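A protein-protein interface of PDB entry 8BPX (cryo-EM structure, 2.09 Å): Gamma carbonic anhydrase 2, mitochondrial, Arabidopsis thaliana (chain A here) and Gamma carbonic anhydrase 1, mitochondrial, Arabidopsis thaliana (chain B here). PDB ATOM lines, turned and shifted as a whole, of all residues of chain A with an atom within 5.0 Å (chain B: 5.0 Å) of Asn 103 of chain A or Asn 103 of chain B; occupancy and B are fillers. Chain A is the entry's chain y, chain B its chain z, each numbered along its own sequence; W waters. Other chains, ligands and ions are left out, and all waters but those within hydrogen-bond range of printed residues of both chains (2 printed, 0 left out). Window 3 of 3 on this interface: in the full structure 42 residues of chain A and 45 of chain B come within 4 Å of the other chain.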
ATOM      1  N   TYR A  81      -0.876  25.292  -4.916  1.00  0.00           N
ATOM      2  CA  TYR A  81      -0.670  24.561  -6.162  1.00  0.00           C
ATOM      3  C   TYR A  81      -1.253  23.153  -6.088  1.00  0.00           C
ATOM      4  O   TYR A  81      -1.011  22.414  -5.130  1.00  0.00           O
ATOM      5  CB  TYR A  81       0.825  24.498  -6.480  1.00  0.00           C
ATOM      6  CG  TYR A  81       1.475  25.862  -6.547  1.00  0.00           C
ATOM      7  CD1 TYR A  81       1.307  26.679  -7.656  1.00  0.00           C
ATOM      8  CD2 TYR A  81       2.222  26.346  -5.482  1.00  0.00           C
ATOM      9  CE1 TYR A  81       1.888  27.929  -7.713  1.00  0.00           C
ATOM     10  CE2 TYR A  81       2.804  27.592  -5.527  1.00  0.00           C
ATOM     11  CZ  TYR A  81       2.633  28.381  -6.644  1.00  0.00           C
ATOM     12  OH  TYR A  81       3.211  29.622  -6.690  1.00  0.00           O
ATOM     13  N   GLY A  82      -2.027  22.787  -7.108  1.00  0.00           N
ATOM     14  CA  GLY A  82      -2.571  21.451  -7.220  1.00  0.00           C
ATOM     15  C   GLY A  82      -3.784  21.164  -6.362  1.00  0.00           C
ATOM     16  O   GLY A  82      -4.281  20.033  -6.388  1.00  0.00           O
ATOM     17  N   CYS A  83      -4.270  22.137  -5.599  1.00  0.00           N
ATOM     18  CA  CYS A  83      -5.464  21.933  -4.790  1.00  0.00           C
ATOM     19  C   CYS A  83      -6.694  21.739  -5.670  1.00  0.00           C
ATOM     20  O   CYS A  83      -6.815  22.328  -6.746  1.00  0.00           O
ATOM     21  CB  CYS A  83      -5.691  23.119  -3.855  1.00  0.00           C
ATOM     22  SG  CYS A  83      -4.362  23.432  -2.694  1.00  0.00           S
ATOM     23  N   VAL A  84      -7.610  20.898  -5.200  1.00  0.00           N
ATOM     24  CA  VAL A  84      -8.888  20.668  -5.863  1.00  0.00           C
ATOM     25  C   VAL A  84      -9.995  20.940  -4.855  1.00  0.00           C
ATOM     26  O   VAL A  84     -10.066  20.282  -3.810  1.00  0.00           O
ATOM     27  CB  VAL A  84      -8.994  19.240  -6.425  1.00  0.00           C
ATOM     28  CG1 VAL A  84     -10.349  19.026  -7.089  1.00  0.00           C
ATOM     29  CG2 VAL A  84      -7.860  18.960  -7.404  1.00  0.00           C
ATOM     30  N   GLN A 101      -3.300  24.051   1.709  1.00  0.00           N
ATOM     31  CA  GLN A 101      -1.952  23.770   1.154  1.00  0.00           C
ATOM     32  C   GLN A 101      -1.904  22.897  -0.121  1.00  0.00           C
ATOM     33  O   GLN A 101      -2.869  22.257  -0.410  1.00  0.00           O
ATOM     34  CB  GLN A 101      -0.996  23.288   2.222  1.00  0.00           C
ATOM     35  CG  GLN A 101      -0.631  24.423   3.184  1.00  0.00           C
ATOM     36  CD  GLN A 101       0.121  23.996   4.420  1.00  0.00           C
ATOM     37  OE1 GLN A 101       0.838  23.007   4.415  1.00  0.00           O
ATOM     38  NE2 GLN A 101      -0.030  24.753   5.496  1.00  0.00           N
ATOM     39  N   ASP A 102      -0.706  22.744  -0.632  1.00  0.00           N
ATOM     40  CA  ASP A 102      -0.551  22.166  -1.962  1.00  0.00           C
ATOM     41  C   ASP A 102      -1.097  20.744  -2.034  1.00  0.00           C
ATOM     42  O   ASP A 102      -0.967  19.961  -1.090  1.00  0.00           O
ATOM     43  CB  ASP A 102       0.927  22.166  -2.352  1.00  0.00           C
ATOM     44  CG  ASP A 102       1.643  23.440  -1.935  1.00  0.00           C
ATOM     45  OD1 ASP A 102       1.917  23.590  -0.727  1.00  0.00           O
ATOM     46  OD2 ASP A 102       1.943  24.278  -2.805  1.00  0.00           O
ATOM     47  N   ASN A 103      -1.717  20.420  -3.170  1.00  0.00           N
ATOM     48  CA  ASN A 103      -2.168  19.072  -3.510  1.00  0.00           C
ATOM     49  C   ASN A 103      -3.260  18.558  -2.571  1.00  0.00           C
ATOM     50  O   ASN A 103      -3.444  17.348  -2.440  1.00  0.00           O
ATOM     51  CB  ASN A 103      -0.992  18.085  -3.544  1.00  0.00           C
ATOM     52  CG  ASN A 103      -0.198  18.155  -4.843  1.00  0.00           C
ATOM     53  OD1 ASN A 103      -0.474  18.980  -5.709  1.00  0.00           O
ATOM     54  ND2 ASN A 103       0.796  17.287  -4.976  1.00  0.00           N
ATOM     55  N   THR A 104      -3.988  19.455  -1.914  1.00  0.00           N
ATOM     56  CA  THR A 104      -5.094  19.066  -1.048  1.00  0.00           C
ATOM     57  C   THR A 104      -6.368  18.857  -1.864  1.00  0.00           C
ATOM     58  O   THR A 104      -6.613  19.543  -2.857  1.00  0.00           O
ATOM     59  CB  THR A 104      -5.320  20.131   0.034  1.00  0.00           C
ATOM     60  OG1 THR A 104      -4.219  20.125   0.952  1.00  0.00           O
ATOM     61  CG2 THR A 104      -6.611  19.891   0.808  1.00  0.00           C
ATOM     62  N   LEU A 105      -7.173  17.885  -1.446  1.00  0.00           N
ATOM     63  CA  LEU A 105      -8.483  17.640  -2.031  1.00  0.00           C
ATOM     64  C   LEU A 105      -9.563  17.984  -1.016  1.00  0.00           C
ATOM     65  O   LEU A 105      -9.542  17.488   0.115  1.00  0.00           O
ATOM     66  CB  LEU A 105      -8.623  16.181  -2.482  1.00  0.00           C
ATOM     67  CG  LEU A 105      -9.928  15.709  -3.143  1.00  0.00           C
ATOM     68  CD1 LEU A 105     -10.979  15.291  -2.113  1.00  0.00           C
ATOM     69  CD2 LEU A 105     -10.490  16.755  -4.105  1.00  0.00           C
ATOM     70  N   SER A 131      -1.472  18.081   0.947  1.00  0.00           N
ATOM     71  CA  SER A 131      -1.992  16.777   0.529  1.00  0.00           C
ATOM     72  C   SER A 131      -2.991  16.199   1.526  1.00  0.00           C
ATOM     73  O   SER A 131      -3.097  14.982   1.678  1.00  0.00           O
ATOM     74  CB  SER A 131      -0.858  15.778   0.284  1.00  0.00           C
ATOM     75  OG  SER A 131       0.000  16.226  -0.746  1.00  0.00           O
ATOM     76  N   ALA A 132      -3.729  17.060   2.217  1.00  0.00           N
ATOM     77  CA  ALA A 132      -4.803  16.580   3.069  1.00  0.00           C
ATOM     78  C   ALA A 132      -6.033  16.256   2.226  1.00  0.00           C
ATOM     79  O   ALA A 132      -6.149  16.663   1.068  1.00  0.00           O
ATOM     80  CB  ALA A 132      -5.151  17.613   4.141  1.00  0.00           C
ATOM     81  N   TYR B  81      -9.809  15.225 -11.517  1.00  0.00           N
ATOM     82  CA  TYR B  81      -8.810  16.285 -11.519  1.00  0.00           C
ATOM     83  C   TYR B  81      -7.572  15.889 -10.722  1.00  0.00           C
ATOM     84  O   TYR B  81      -7.669  15.410  -9.591  1.00  0.00           O
ATOM     85  CB  TYR B  81      -9.430  17.565 -10.957  1.00  0.00           C
ATOM     86  CG  TYR B  81     -10.636  18.031 -11.746  1.00  0.00           C
ATOM     87  CD1 TYR B  81     -10.492  18.875 -12.839  1.00  0.00           C
ATOM     88  CD2 TYR B  81     -11.919  17.609 -11.408  1.00  0.00           C
ATOM     89  CE1 TYR B  81     -11.588  19.294 -13.567  1.00  0.00           C
ATOM     90  CE2 TYR B  81     -13.019  18.020 -12.132  1.00  0.00           C
ATOM     91  CZ  TYR B  81     -12.851  18.862 -13.211  1.00  0.00           C
ATOM     92  OH  TYR B  81     -13.945  19.277 -13.930  1.00  0.00           O
ATOM     93  N   GLY B  82      -6.402  16.084 -11.329  1.00  0.00           N
ATOM     94  CA  GLY B  82      -5.134  15.822 -10.683  1.00  0.00           C
ATOM     95  C   GLY B  82      -4.672  14.381 -10.698  1.00  0.00           C
ATOM     96  O   GLY B  82      -3.600  14.089 -10.154  1.00  0.00           O
ATOM     97  N   CYS B  83      -5.437  13.471 -11.294  1.00  0.00           N
ATOM     98  CA  CYS B  83      -5.057  12.066 -11.312  1.00  0.00           C
ATOM     99  C   CYS B  83      -3.815  11.839 -12.166  1.00  0.00           C
ATOM    100  O   CYS B  83      -3.561  12.550 -13.141  1.00  0.00           O
ATOM    101  CB  CYS B  83      -6.202  11.207 -11.840  1.00  0.00           C
ATOM    102  SG  CYS B  83      -7.627  11.122 -10.757  1.00  0.00           S
ATOM    103  N   GLN B 101     -10.912   8.810  -8.679  1.00  0.00           N
ATOM    104  CA  GLN B 101     -11.164  10.120  -8.051  1.00  0.00           C
ATOM    105  C   GLN B 101      -9.993  11.099  -7.970  1.00  0.00           C
ATOM    106  O   GLN B 101      -8.886  10.686  -8.069  1.00  0.00           O
ATOM    107  CB  GLN B 101     -11.952   9.908  -6.770  1.00  0.00           C
ATOM    108  CG  GLN B 101     -13.378   9.438  -7.055  1.00  0.00           C
ATOM    109  CD  GLN B 101     -14.099   9.156  -5.764  1.00  0.00           C
ATOM    110  OE1 GLN B 101     -13.701   9.646  -4.721  1.00  0.00           O
ATOM    111  NE2 GLN B 101     -15.158   8.368  -5.820  1.00  0.00           N
ATOM    112  N   ASP B 102     -10.314  12.308  -7.586  1.00  0.00           N
ATOM    113  CA  ASP B 102      -9.327  13.374  -7.710  1.00  0.00           C
ATOM    114  C   ASP B 102      -8.036  13.062  -6.965  1.00  0.00           C
ATOM    115  O   ASP B 102      -8.051  12.546  -5.845  1.00  0.00           O
ATOM    116  CB  ASP B 102      -9.907  14.690  -7.190  1.00  0.00           C
ATOM    117  CG  ASP B 102     -10.973  15.260  -8.101  1.00  0.00           C
ATOM    118  OD1 ASP B 102     -11.070  14.809  -9.257  1.00  0.00           O
ATOM    119  OD2 ASP B 102     -11.710  16.164  -7.663  1.00  0.00           O
ATOM    120  N   ASN B 103      -6.927  13.362  -7.640  1.00  0.00           N
ATOM    121  CA  ASN B 103      -5.571  13.241  -7.015  1.00  0.00           C
ATOM    122  C   ASN B 103      -5.153  11.788  -6.748  1.00  0.00           C
ATOM    123  O   ASN B 103      -4.213  11.595  -6.071  1.00  0.00           O
ATOM    124  CB  ASN B 103      -5.403  14.131  -5.763  1.00  0.00           C
ATOM    125  CG  ASN B 103      -5.585  15.616  -6.035  1.00  0.00           C
ATOM    126  OD1 ASN B 103      -5.597  16.061  -7.180  1.00  0.00           O
ATOM    127  ND2 ASN B 103      -5.720  16.408  -4.984  1.00  0.00           N
ATOM    128  N   SER B 104      -5.837  10.843  -7.344  1.00  0.00           N
ATOM    129  CA  SER B 104      -5.421   9.457  -7.204  1.00  0.00           C
ATOM    130  C   SER B 104      -4.229   9.161  -8.110  1.00  0.00           C
ATOM    131  O   SER B 104      -3.987   9.846  -9.105  1.00  0.00           O
ATOM    132  CB  SER B 104      -6.572   8.510  -7.534  1.00  0.00           C
ATOM    133  OG  SER B 104      -7.515   8.483  -6.483  1.00  0.00           O
ATOM    134  N   LEU B 105      -3.475   8.126  -7.720  1.00  0.00           N
ATOM    135  CA  LEU B 105      -2.282   7.699  -8.458  1.00  0.00           C
ATOM    136  C   LEU B 105      -2.369   6.192  -8.799  1.00  0.00           C
ATOM    137  O   LEU B 105      -2.413   5.390  -7.884  1.00  0.00           O
ATOM    138  CB  LEU B 105      -1.015   8.040  -7.684  1.00  0.00           C
ATOM    139  CG  LEU B 105       0.297   7.473  -8.225  1.00  0.00           C
ATOM    140  CD1 LEU B 105       0.671   8.100  -9.560  1.00  0.00           C
ATOM    141  CD2 LEU B 105       1.421   7.668  -7.219  1.00  0.00           C
ATOM    142  N   SER B 131      -7.266  10.476  -3.801  1.00  0.00           N
ATOM    143  CA  SER B 131      -5.879  10.398  -3.294  1.00  0.00           C
ATOM    144  C   SER B 131      -5.470   8.977  -2.894  1.00  0.00           C
ATOM    145  O   SER B 131      -4.653   8.847  -2.081  1.00  0.00           O
ATOM    146  CB  SER B 131      -5.652  11.443  -2.171  1.00  0.00           C
ATOM    147  OG  SER B 131      -6.214  12.706  -2.497  1.00  0.00           O
ATOM    148  N   ALA B 132      -6.083   8.023  -3.522  1.00  0.00           N
ATOM    149  CA  ALA B 132      -5.659   6.646  -3.345  1.00  0.00           C
ATOM    150  C   ALA B 132      -4.429   6.361  -4.199  1.00  0.00           C
ATOM    151  O   ALA B 132      -4.181   7.015  -5.215  1.00  0.00           O
ATOM    152  CB  ALA B 132      -6.790   5.682  -3.707  1.00  0.00           C
HETATM  153  O   HOH W   1      -4.947  15.150  -1.515  1.00  0.00           O
HETATM  154  O   HOH W   2      -4.071  18.579  -8.934  1.00  0.00           O
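O of Tyr 81 of chain A sits at hydrogen-bond distance from N of Asn 103 of chain A, at 2.9 Å. The side-chain carboxylate of Asp 102 of chain B lies within hydrogen-bond range of the backbone NH of Tyr 81 of chain B. The backbone carbonyl oxygen of Asp 102 of chain B sits at hydrogen-bond distance from the backbone NH of Ser 131 of chain B (3.0 Å). The backbone NH of Leu 105 of chain A is in hydrogen-bond range of the backbone carbonyl oxygen of Ala 132 of chain A (3.0 Å). The backbone NH (N) of Val 84 of chain A lies within hydrogen-bond range of the backbone carbonyl oxygen (O) of Thr 104 of chain A (2.9 Å). The backbone NH of Ser 131 of chain A lies within hydrogen-bond range of the side-chain hydroxyl of Thr 104 of chain A (3.4 Å).
Among the printed residues, merely in contact across the chains: Val 84 of chain A with Asp 102 of chain B, Asn 103 of chain A with Asn 103 of chain B, Val 84 of chain A with Asn 103 of chain B, Leu 105 of chain A with Asp 102 of chain B, Leu 105 of chain A with Asn 103 of chain B and Thr 104 of chain A with Asn 103 of chain B.
Of the printed residues of chain B, Val 84 of chain A touches Asp 102 (3.2 Å) and Asn 103 (3.7 Å). Asn 103 of chain A touches just one residue of chain B: Asn 103. Ser 131 of chain A touches none of the printed residues of chain B. Tyr 81 of chain B touches none of the printed residues of chain A. Printed residues of chain A within 4 Å of Asp 102 of chain B: Val 84 and Leu 105. The nearest residue of chain A that does not touch Asn 103 of chain B is Gly 82 of chain A (4.1 Å).
Of the 10 printed residues of chain B, 2 touch a printed residue of chain A. Printed residues of chain B that touch a printed residue of chain A: Asp 102 and Asn 103. Along chain B the printed residues that touch a printed residue of chain A span positions 102 to 103. Of the 11 printed residues of chain A, 4 touch a printed residue of chain B. Hydrophobic or aromatic side chains of chain A that line the printed part of chain B: Val 84 and Leu 105. Among the printed residues, no Asp or Glu carboxylate lies within 4 Å of a Lys or Arg side-chain nitrogen of the other chain.
Water W1 lies within hydrogen-bond range of the backbone carbonyl oxygen of Asn 103 of chain A, the side-chain hydroxyl of Ser 131 of chain B and the backbone carbonyl oxygen of Ala 132 of chain A. Water W2 bridges O of Gly 82 of chain A and OD1 of Asn 103 of chain B.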
